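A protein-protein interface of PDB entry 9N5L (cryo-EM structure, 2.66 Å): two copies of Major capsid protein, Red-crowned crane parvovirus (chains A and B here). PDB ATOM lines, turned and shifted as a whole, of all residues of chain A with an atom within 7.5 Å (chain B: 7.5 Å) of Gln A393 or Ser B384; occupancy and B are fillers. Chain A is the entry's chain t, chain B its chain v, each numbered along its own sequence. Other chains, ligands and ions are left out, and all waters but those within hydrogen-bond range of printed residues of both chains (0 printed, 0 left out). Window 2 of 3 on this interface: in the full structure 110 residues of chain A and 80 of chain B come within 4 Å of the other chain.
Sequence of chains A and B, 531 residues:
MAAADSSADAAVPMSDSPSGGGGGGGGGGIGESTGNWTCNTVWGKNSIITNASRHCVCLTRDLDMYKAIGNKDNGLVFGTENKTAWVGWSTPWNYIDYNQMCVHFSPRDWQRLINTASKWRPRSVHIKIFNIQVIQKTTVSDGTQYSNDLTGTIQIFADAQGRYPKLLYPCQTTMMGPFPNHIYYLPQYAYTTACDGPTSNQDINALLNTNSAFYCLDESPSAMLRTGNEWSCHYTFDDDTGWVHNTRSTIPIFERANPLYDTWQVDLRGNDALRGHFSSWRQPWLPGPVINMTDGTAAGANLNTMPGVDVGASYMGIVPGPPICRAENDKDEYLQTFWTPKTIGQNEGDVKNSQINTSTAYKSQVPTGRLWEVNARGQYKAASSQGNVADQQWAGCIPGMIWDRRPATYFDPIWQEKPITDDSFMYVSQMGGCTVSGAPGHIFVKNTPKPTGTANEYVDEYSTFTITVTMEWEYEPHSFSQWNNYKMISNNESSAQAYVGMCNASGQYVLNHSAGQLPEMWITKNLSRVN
Ile A291 touches Ala B382.
Asn A292 touches Ala B382.
Ala B383 touches Thr A294 (CB to CB, 3.4 Å).
Thr A294 touches Gly B387 (OG1 to CA, 3.0 Å).
CG2 of Thr A294 touches CG1 of Val B389, 3.6 Å away.
Pro A307 touches Val B389 (N to CG1, 3.5 Å).
O of Gln A393 touches CB of Ala B382, at 3.9 Å.
CG of Gln A393 touches O of Ala B383, 3.6 Å away.
Gln A393 touches Ala B390.
Trp A394 touches Tyr B380.
Among the printed residues, no Asp or Glu carboxylate lies within 4 Å of a Lys or Arg side-chain nitrogen of the other chain.
Gln A393 touches Gln B392, but with the chains exchanged Gln A392 does not touch Gln B393 (8.6 Å).
Trp A394 touches Tyr B380, but with the chains exchanged Tyr A380 does not touch Trp B394 (11.6 Å).
Trp A394 touches Gln B392, but with the chains exchanged Gln A392 does not touch Trp B394 (7.4 Å).
Trp A394 touches its own counterpart, Trp B394.
6 positions are printed for both chains.
Printed residues of chain B within 4 Å of Asn A292: Ala B382, Ala B383 and Ser B384.
Printed residues of chain A within 4 Å of Ala B382: Ile A291 (3.9 Å), Asn A292 (3.7 Å), Pro A307 (3.7 Å) and Gln A393 (3.9 Å).
Of chain A, only Asn A292 (3.0 Å) and Gln A393 (3.0 Å) come within 4 Å of Ser B384.
Printed residues of chain A within 4 Å of Val B389: Thr A294 (3.6 Å) and Pro A307 (3.5 Å).
Printed residues of chain A within 4 Å of Ala B390: Gln A393.
The nearest residue of chain B that does not touch Gln A393 is Asp B391 (4.6 Å).
The nearest printed residue of chain A that does not touch Val B389 is Gln A393 (6.4 Å).
N of Ala B383 is in hydrogen-bond range of O of Asn A292, 3.3 Å away.
O of Ser B384 lies within hydrogen-bond range of ND2 of Asn A292 (3.0 Å).
OE1 of Gln A393 sits at hydrogen-bond distance from NE2 of Gln B392, 3.0 Å away.
ND2 of Asn A292 lies close to OE1 of Gln A379.
The backbone NH (N) of Asn A292 lies within hydrogen-bond range of the backbone carbonyl oxygen (O) of Gln A393.
The backbone NH (N) of Ile A318 lies within hydrogen-bond range of the backbone carbonyl oxygen (O) of Pro A307, 3.2 Å away.
O of Tyr B380 is in hydrogen-bond range of N of Gln B392.
OG of Ser B384 is in hydrogen-bond range of O of Asn B388 (3.3 Å).
The backbone carbonyl oxygen (O) of Ala B390 sits at hydrogen-bond distance from the side-chain amide nitrogen (NE2) of Gln B392 (3.1 Å).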
ATOM      1  N   VAL A 290      -1.751  35.524  -9.673  1.00  0.00           N
ATOM      2  CA  VAL A 290      -0.402  35.252  -9.235  1.00  0.00           C
ATOM      3  C   VAL A 290       0.166  34.071  -9.991  1.00  0.00           C
ATOM      4  O   VAL A 290      -0.447  33.015 -10.045  1.00  0.00           O
ATOM      5  CB  VAL A 290      -0.363  34.917  -7.737  1.00  0.00           C
ATOM      6  CG1 VAL A 290       1.059  34.599  -7.301  1.00  0.00           C
ATOM      7  CG2 VAL A 290      -0.940  36.062  -6.925  1.00  0.00           C
ATOM      8  N   ILE A 291       1.322  34.258 -10.600  1.00  0.00           N
ATOM      9  CA  ILE A 291       1.963  33.173 -11.312  1.00  0.00           C
ATOM     10  C   ILE A 291       3.146  32.835 -10.443  1.00  0.00           C
ATOM     11  O   ILE A 291       3.902  33.719 -10.069  1.00  0.00           O
ATOM     12  CB  ILE A 291       2.468  33.594 -12.699  1.00  0.00           C
ATOM     13  CG1 ILE A 291       1.325  34.151 -13.546  1.00  0.00           C
ATOM     14  CG2 ILE A 291       3.125  32.422 -13.400  1.00  0.00           C
ATOM     15  CD1 ILE A 291       0.043  33.365 -13.431  1.00  0.00           C
ATOM     16  N   ASN A 292       3.307  31.565 -10.103  1.00  0.00           N
ATOM     17  CA  ASN A 292       4.419  31.188  -9.257  1.00  0.00           C
ATOM     18  C   ASN A 292       5.699  31.524  -9.996  1.00  0.00           C
ATOM     19  O   ASN A 292       5.842  31.243 -11.178  1.00  0.00           O
ATOM     20  CB  ASN A 292       4.369  29.704  -8.921  1.00  0.00           C
ATOM     21  CG  ASN A 292       5.243  29.349  -7.742  1.00  0.00           C
ATOM     22  OD1 ASN A 292       5.705  30.223  -7.019  1.00  0.00           O
ATOM     23  ND2 ASN A 292       5.472  28.065  -7.540  1.00  0.00           N
ATOM     24  N   MET A 293       6.641  32.113  -9.279  1.00  0.00           N
ATOM     25  CA  MET A 293       7.892  32.517  -9.882  1.00  0.00           C
ATOM     26  C   MET A 293       9.034  31.931  -9.083  1.00  0.00           C
ATOM     27  O   MET A 293       8.925  31.735  -7.878  1.00  0.00           O
ATOM     28  CB  MET A 293       7.987  34.040  -9.912  1.00  0.00           C
ATOM     29  CG  MET A 293       8.518  34.610 -11.215  1.00  0.00           C
ATOM     30  SD  MET A 293       7.392  34.387 -12.604  1.00  0.00           S
ATOM     31  CE  MET A 293       5.969  35.323 -12.067  1.00  0.00           C
ATOM     32  N   THR A 294      10.123  31.626  -9.769  1.00  0.00           N
ATOM     33  CA  THR A 294      11.284  31.053  -9.122  1.00  0.00           C
ATOM     34  C   THR A 294      12.544  31.739  -9.605  1.00  0.00           C
ATOM     35  O   THR A 294      12.555  32.362 -10.661  1.00  0.00           O
ATOM     36  CB  THR A 294      11.403  29.549  -9.407  1.00  0.00           C
ATOM     37  OG1 THR A 294      12.428  28.986  -8.580  1.00  0.00           O
ATOM     38  CG2 THR A 294      11.750  29.310 -10.864  1.00  0.00           C
ATOM     39  N   PRO A 307      10.591  30.394 -15.146  1.00  0.00           N
ATOM     40  CA  PRO A 307       9.220  30.425 -15.656  1.00  0.00           C
ATOM     41  C   PRO A 307       9.138  31.242 -16.933  1.00  0.00           C
ATOM     42  O   PRO A 307       9.659  32.349 -17.009  1.00  0.00           O
ATOM     43  CB  PRO A 307       8.438  31.119 -14.534  1.00  0.00           C
ATOM     44  CG  PRO A 307       9.460  31.753 -13.657  1.00  0.00           C
ATOM     45  CD  PRO A 307      10.693  30.920 -13.778  1.00  0.00           C
ATOM     46  N   ILE A 318       8.438  34.989 -18.374  1.00  0.00           N
ATOM     47  CA  ILE A 318       7.371  35.814 -17.828  1.00  0.00           C
ATOM     48  C   ILE A 318       7.765  36.526 -16.546  1.00  0.00           C
ATOM     49  O   ILE A 318       6.948  37.257 -15.979  1.00  0.00           O
ATOM     50  CB  ILE A 318       6.106  34.970 -17.611  1.00  0.00           C
ATOM     51  CG1 ILE A 318       6.429  33.781 -16.717  1.00  0.00           C
ATOM     52  CG2 ILE A 318       5.556  34.507 -18.937  1.00  0.00           C
ATOM     53  CD1 ILE A 318       5.245  32.964 -16.366  1.00  0.00           C
ATOM     54  N   GLN A 379       1.478  33.001  -3.890  1.00  0.00           N
ATOM     55  CA  GLN A 379       0.661  32.252  -4.829  1.00  0.00           C
ATOM     56  C   GLN A 379      -0.563  31.673  -4.138  1.00  0.00           C
ATOM     57  O   GLN A 379      -0.490  31.206  -3.008  1.00  0.00           O
ATOM     58  CB  GLN A 379       1.475  31.114  -5.431  1.00  0.00           C
ATOM     59  CG  GLN A 379       2.079  30.205  -4.385  1.00  0.00           C
ATOM     60  CD  GLN A 379       2.851  29.062  -4.989  1.00  0.00           C
ATOM     61  OE1 GLN A 379       2.575  28.636  -6.106  1.00  0.00           O
ATOM     62  NE2 GLN A 379       3.825  28.554  -4.249  1.00  0.00           N
ATOM     63  N   TYR A 380      -1.687  31.707  -4.842  1.00  0.00           N
ATOM     64  CA  TYR A 380      -2.961  31.218  -4.336  1.00  0.00           C
ATOM     65  C   TYR A 380      -3.052  29.731  -4.070  1.00  0.00           C
ATOM     66  O   TYR A 380      -2.463  28.923  -4.776  1.00  0.00           O
ATOM     67  CB  TYR A 380      -4.058  31.458  -5.377  1.00  0.00           C
ATOM     68  CG  TYR A 380      -4.464  32.880  -5.645  1.00  0.00           C
ATOM     69  CD1 TYR A 380      -5.598  33.415  -5.060  1.00  0.00           C
ATOM     70  CD2 TYR A 380      -3.745  33.669  -6.525  1.00  0.00           C
ATOM     71  CE1 TYR A 380      -5.988  34.712  -5.318  1.00  0.00           C
ATOM     72  CE2 TYR A 380      -4.126  34.967  -6.788  1.00  0.00           C
ATOM     73  CZ  TYR A 380      -5.248  35.482  -6.182  1.00  0.00           C
ATOM     74  OH  TYR A 380      -5.626  36.772  -6.447  1.00  0.00           O
ATOM     75  N   ALA A 390      -4.002  23.239  -2.810  1.00  0.00           N
ATOM     76  CA  ALA A 390      -2.628  23.225  -3.269  1.00  0.00           C
ATOM     77  C   ALA A 390      -2.240  24.612  -3.742  1.00  0.00           C
ATOM     78  O   ALA A 390      -3.084  25.395  -4.181  1.00  0.00           O
ATOM     79  CB  ALA A 390      -2.424  22.221  -4.403  1.00  0.00           C
ATOM     80  N   ASP A 391      -0.951  24.906  -3.639  1.00  0.00           N
ATOM     81  CA  ASP A 391      -0.424  26.141  -4.189  1.00  0.00           C
ATOM     82  C   ASP A 391      -0.626  26.176  -5.694  1.00  0.00           C
ATOM     83  O   ASP A 391      -0.351  25.201  -6.396  1.00  0.00           O
ATOM     84  CB  ASP A 391       1.053  26.263  -3.856  1.00  0.00           C
ATOM     85  CG  ASP A 391       1.292  26.614  -2.413  1.00  0.00           C
ATOM     86  OD1 ASP A 391       0.351  27.089  -1.752  1.00  0.00           O
ATOM     87  OD2 ASP A 391       2.428  26.421  -1.943  1.00  0.00           O
ATOM     88  N   GLN A 392      -1.105  27.305  -6.194  1.00  0.00           N
ATOM     89  CA  GLN A 392      -1.427  27.438  -7.605  1.00  0.00           C
ATOM     90  C   GLN A 392      -0.226  28.003  -8.343  1.00  0.00           C
ATOM     91  O   GLN A 392       0.146  29.163  -8.143  1.00  0.00           O
ATOM     92  CB  GLN A 392      -2.656  28.315  -7.801  1.00  0.00           C
ATOM     93  CG  GLN A 392      -3.884  27.676  -7.220  1.00  0.00           C
ATOM     94  CD  GLN A 392      -4.133  26.315  -7.812  1.00  0.00           C
ATOM     95  OE1 GLN A 392      -4.028  26.125  -9.021  1.00  0.00           O
ATOM     96  NE2 GLN A 392      -4.426  25.345  -6.962  1.00  0.00           N
ATOM     97  N   GLN A 393       0.368  27.178  -9.202  1.00  0.00           N
ATOM     98  CA  GLN A 393       1.557  27.595  -9.928  1.00  0.00           C
ATOM     99  C   GLN A 393       1.226  28.702 -10.912  1.00  0.00           C
ATOM    100  O   GLN A 393       2.002  29.648 -11.082  1.00  0.00           O
ATOM    101  CB  GLN A 393       2.151  26.394 -10.652  1.00  0.00           C
ATOM    102  CG  GLN A 393       2.485  25.256  -9.730  1.00  0.00           C
ATOM    103  CD  GLN A 393       2.881  24.020 -10.480  1.00  0.00           C
ATOM    104  OE1 GLN A 393       2.619  23.901 -11.673  1.00  0.00           O
ATOM    105  NE2 GLN A 393       3.463  23.062  -9.777  1.00  0.00           N
ATOM    106  N   TRP A 394       0.078  28.602 -11.570  1.00  0.00           N
ATOM    107  CA  TRP A 394      -0.417  29.640 -12.459  1.00  0.00           C
ATOM    108  C   TRP A 394      -1.831  29.964 -12.015  1.00  0.00           C
ATOM    109  O   TRP A 394      -2.715  29.111 -12.112  1.00  0.00           O
ATOM    110  CB  TRP A 394      -0.443  29.174 -13.915  1.00  0.00           C
ATOM    111  CG  TRP A 394      -0.700  30.274 -14.873  1.00  0.00           C
ATOM    112  CD1 TRP A 394      -1.897  30.821 -15.181  1.00  0.00           C
ATOM    113  CD2 TRP A 394       0.247  30.868 -15.755  1.00  0.00           C
ATOM    114  NE1 TRP A 394      -1.748  31.791 -16.135  1.00  0.00           N
ATOM    115  CE2 TRP A 394      -0.436  31.828 -16.514  1.00  0.00           C
ATOM    116  CE3 TRP A 394       1.618  30.711 -15.947  1.00  0.00           C
ATOM    117  CZ2 TRP A 394       0.201  32.618 -17.453  1.00  0.00           C
ATOM    118  CZ3 TRP A 394       2.241  31.491 -16.871  1.00  0.00           C
ATOM    119  CH2 TRP A 394       1.540  32.435 -17.613  1.00  0.00           C
ATOM    120  N   ALA A 395      -2.051  31.171 -11.523  1.00  0.00           N
ATOM    121  CA  ALA A 395      -3.400  31.622 -11.203  1.00  0.00           C
ATOM    122  C   ALA A 395      -3.719  32.752 -12.163  1.00  0.00           C
ATOM    123  O   ALA A 395      -3.246  33.875 -11.986  1.00  0.00           O
ATOM    124  CB  ALA A 395      -3.505  32.070  -9.753  1.00  0.00           C
ATOM    125  N   GLY A 396      -4.550  32.467 -13.153  1.00  0.00           N
ATOM    126  CA  GLY A 396      -4.876  33.466 -14.142  1.00  0.00           C
ATOM    127  C   GLY A 396      -5.984  34.379 -13.674  1.00  0.00           C
ATOM    128  O   GLY A 396      -6.556  34.215 -12.601  1.00  0.00           O
ATOM    129  N   TYR B 380       3.344  26.942 -21.033  1.00  0.00           N
ATOM    130  CA  TYR B 380       4.246  27.658 -20.142  1.00  0.00           C
ATOM    131  C   TYR B 380       4.791  26.872 -18.967  1.00  0.00           C
ATOM    132  O   TYR B 380       4.115  26.024 -18.402  1.00  0.00           O
ATOM    133  CB  TYR B 380       3.502  28.817 -19.475  1.00  0.00           C
ATOM    134  CG  TYR B 380       3.096  29.974 -20.343  1.00  0.00           C
ATOM    135  CD1 TYR B 380       3.850  31.134 -20.377  1.00  0.00           C
ATOM    136  CD2 TYR B 380       1.932  29.929 -21.089  1.00  0.00           C
ATOM    137  CE1 TYR B 380       3.474  32.207 -21.155  1.00  0.00           C
ATOM    138  CE2 TYR B 380       1.547  30.997 -21.871  1.00  0.00           C
ATOM    139  CZ  TYR B 380       2.321  32.132 -21.898  1.00  0.00           C
ATOM    140  OH  TYR B 380       1.935  33.192 -22.678  1.00  0.00           O
ATOM    141  N   LYS B 381       6.038  27.157 -18.623  1.00  0.00           N
ATOM    142  CA  LYS B 381       6.623  26.645 -17.402  1.00  0.00           C
ATOM    143  C   LYS B 381       6.534  27.749 -16.364  1.00  0.00           C
ATOM    144  O   LYS B 381       6.806  28.911 -16.666  1.00  0.00           O
ATOM    145  CB  LYS B 381       8.064  26.198 -17.622  1.00  0.00           C
ATOM    146  CG  LYS B 381       8.156  24.985 -18.515  1.00  0.00           C
ATOM    147  CD  LYS B 381       9.579  24.586 -18.780  1.00  0.00           C
ATOM    148  CE  LYS B 381       9.635  23.348 -19.642  1.00  0.00           C
ATOM    149  NZ  LYS B 381      11.032  22.972 -19.966  1.00  0.00           N
ATOM    150  N   ALA B 382       6.086  27.395 -15.170  1.00  0.00           N
ATOM    151  CA  ALA B 382       6.075  28.307 -14.044  1.00  0.00           C
ATOM    152  C   ALA B 382       6.605  27.554 -12.841  1.00  0.00           C
ATOM    153  O   ALA B 382       6.595  26.323 -12.816  1.00  0.00           O
ATOM    154  CB  ALA B 382       4.680  28.854 -13.750  1.00  0.00           C
ATOM    155  N   ALA B 383       7.074  28.303 -11.851  1.00  0.00           N
ATOM    156  CA  ALA B 383       7.700  27.686 -10.694  1.00  0.00           C
ATOM    157  C   ALA B 383       6.740  26.720 -10.023  1.00  0.00           C
ATOM    158  O   ALA B 383       5.608  27.076  -9.695  1.00  0.00           O
ATOM    159  CB  ALA B 383       8.150  28.752  -9.707  1.00  0.00           C
ATOM    160  N   SER B 384       7.158  25.481  -9.826  1.00  0.00           N
ATOM    161  CA  SER B 384       6.263  24.563  -9.158  1.00  0.00           C
ATOM    162  C   SER B 384       6.582  24.622  -7.679  1.00  0.00           C
ATOM    163  O   SER B 384       5.784  25.107  -6.883  1.00  0.00           O
ATOM    164  CB  SER B 384       6.462  23.146  -9.686  1.00  0.00           C
ATOM    165  OG  SER B 384       7.796  22.717  -9.496  1.00  0.00           O
ATOM    166  N   SER B 385       7.772  24.158  -7.324  1.00  0.00           N
ATOM    167  CA  SER B 385       8.227  24.180  -5.945  1.00  0.00           C
ATOM    168  C   SER B 385       9.729  23.995  -5.920  1.00  0.00           C
ATOM    169  O   SER B 385      10.303  23.529  -6.892  1.00  0.00           O
ATOM    170  CB  SER B 385       7.562  23.060  -5.149  1.00  0.00           C
ATOM    171  OG  SER B 385       7.939  21.794  -5.662  1.00  0.00           O
ATOM    172  N   GLN B 386      10.365  24.404  -4.827  1.00  0.00           N
ATOM    173  CA  GLN B 386      11.803  24.209  -4.630  1.00  0.00           C
ATOM    174  C   GLN B 386      12.689  24.662  -5.794  1.00  0.00           C
ATOM    175  O   GLN B 386      13.604  23.948  -6.202  1.00  0.00           O
ATOM    176  CB  GLN B 386      12.122  22.780  -4.151  1.00  0.00           C
ATOM    177  CG  GLN B 386      12.385  21.742  -5.228  1.00  0.00           C
ATOM    178  CD  GLN B 386      11.977  20.347  -4.799  1.00  0.00           C
ATOM    179  OE1 GLN B 386      11.158  20.177  -3.894  1.00  0.00           O
ATOM    180  NE2 GLN B 386      12.539  19.338  -5.454  1.00  0.00           N
ATOM    181  N   GLY B 387      12.428  25.856  -6.312  1.00  0.00           N
ATOM    182  CA  GLY B 387      13.199  26.383  -7.421  1.00  0.00           C
ATOM    183  C   GLY B 387      13.146  25.542  -8.683  1.00  0.00           C
ATOM    184  O   GLY B 387      14.143  25.388  -9.381  1.00  0.00           O
ATOM    185  N   ASN B 388      11.971  24.994  -8.968  1.00  0.00           N
ATOM    186  CA  ASN B 388      11.753  24.184 -10.155  1.00  0.00           C
ATOM    187  C   ASN B 388      10.561  24.751 -10.899  1.00  0.00           C
ATOM    188  O   ASN B 388       9.680  25.353 -10.298  1.00  0.00           O
ATOM    189  CB  ASN B 388      11.462  22.733  -9.786  1.00  0.00           C
ATOM    190  CG  ASN B 388      12.665  22.022  -9.213  1.00  0.00           C
ATOM    191  OD1 ASN B 388      13.804  22.369  -9.507  1.00  0.00           O
ATOM    192  ND2 ASN B 388      12.416  21.010  -8.394  1.00  0.00           N
ATOM    193  N   VAL B 389      10.539  24.571 -12.211  1.00  0.00           N
ATOM    194  CA  VAL B 389       9.441  25.056 -13.028  1.00  0.00           C
ATOM    195  C   VAL B 389       8.732  23.868 -13.640  1.00  0.00           C
ATOM    196  O   VAL B 389       9.369  22.936 -14.119  1.00  0.00           O
ATOM    197  CB  VAL B 389       9.914  25.986 -14.155  1.00  0.00           C
ATOM    198  CG1 VAL B 389      10.385  27.313 -13.590  1.00  0.00           C
ATOM    199  CG2 VAL B 389      11.005  25.316 -14.970  1.00  0.00           C
ATOM    200  N   ALA B 390       7.409  23.891 -13.592  1.00  0.00           N
ATOM    201  CA  ALA B 390       6.617  22.808 -14.140  1.00  0.00           C
ATOM    202  C   ALA B 390       5.816  23.317 -15.323  1.00  0.00           C
ATOM    203  O   ALA B 390       5.479  24.500 -15.401  1.00  0.00           O
ATOM    204  CB  ALA B 390       5.671  22.219 -13.096  1.00  0.00           C
ATOM    205  N   ASP B 391       5.524  22.410 -16.244  1.00  0.00           N
ATOM    206  CA  ASP B 391       4.641  22.728 -17.349  1.00  0.00           C
ATOM    207  C   ASP B 391       3.260  23.095 -16.832  1.00  0.00           C
ATOM    208  O   ASP B 391       2.700  22.411 -15.975  1.00  0.00           O
ATOM    209  CB  ASP B 391       4.549  21.543 -18.293  1.00  0.00           C
ATOM    210  CG  ASP B 391       5.792  21.367 -19.123  1.00  0.00           C
ATOM    211  OD1 ASP B 391       6.578  22.326 -19.227  1.00  0.00           O
ATOM    212  OD2 ASP B 391       5.977  20.270 -19.679  1.00  0.00           O
ATOM    213  N   GLN B 392       2.708  24.177 -17.359  1.00  0.00           N
ATOM    214  CA  GLN B 392       1.430  24.686 -16.889  1.00  0.00           C
ATOM    215  C   GLN B 392       0.314  24.102 -17.737  1.00  0.00           C
ATOM    216  O   GLN B 392       0.196  24.418 -18.925  1.00  0.00           O
ATOM    217  CB  GLN B 392       1.407  26.209 -16.921  1.00  0.00           C
ATOM    218  CG  GLN B 392       2.394  26.792 -15.953  1.00  0.00           C
ATOM    219  CD  GLN B 392       2.143  26.311 -14.549  1.00  0.00           C
ATOM    220  OE1 GLN B 392       1.005  26.265 -14.092  1.00  0.00           O
ATOM    221  NE2 GLN B 392       3.202  25.910 -13.864  1.00  0.00           N
ATOM    222  N   GLN B 393      -0.506  23.258 -17.116  1.00  0.00           N
ATOM    223  CA  GLN B 393      -1.580  22.599 -17.841  1.00  0.00           C
ATOM    224  C   GLN B 393      -2.627  23.606 -18.283  1.00  0.00           C
ATOM    225  O   GLN B 393      -3.163  23.515 -19.392  1.00  0.00           O
ATOM    226  CB  GLN B 393      -2.206  21.530 -16.955  1.00  0.00           C
ATOM    227  CG  GLN B 393      -1.213  20.513 -16.472  1.00  0.00           C
ATOM    228  CD  GLN B 393      -1.803  19.589 -15.449  1.00  0.00           C
ATOM    229  OE1 GLN B 393      -2.844  19.882 -14.870  1.00  0.00           O
ATOM    230  NE2 GLN B 393      -1.115  18.494 -15.173  1.00  0.00           N
ATOM    231  N   TRP B 394      -2.933  24.574 -17.427  1.00  0.00           N
ATOM    232  CA  TRP B 394      -3.835  25.666 -17.758  1.00  0.00           C
ATOM    233  C   TRP B 394      -3.102  26.954 -17.436  1.00  0.00           C
ATOM    234  O   TRP B 394      -2.809  27.218 -16.269  1.00  0.00           O
ATOM    235  CB  TRP B 394      -5.124  25.603 -16.938  1.00  0.00           C
ATOM    236  CG  TRP B 394      -6.165  26.542 -17.418  1.00  0.00           C
ATOM    237  CD1 TRP B 394      -6.243  27.868 -17.166  1.00  0.00           C
ATOM    238  CD2 TRP B 394      -7.355  26.199 -18.121  1.00  0.00           C
ATOM    239  NE1 TRP B 394      -7.362  28.399 -17.748  1.00  0.00           N
ATOM    240  CE2 TRP B 394      -8.071  27.386 -18.330  1.00  0.00           C
ATOM    241  CE3 TRP B 394      -7.867  25.008 -18.628  1.00  0.00           C
ATOM    242  CZ2 TRP B 394      -9.270  27.416 -19.018  1.00  0.00           C
ATOM    243  CZ3 TRP B 394      -9.047  25.042 -19.305  1.00  0.00           C
ATOM    244  CH2 TRP B 394      -9.740  26.232 -19.497  1.00  0.00           C
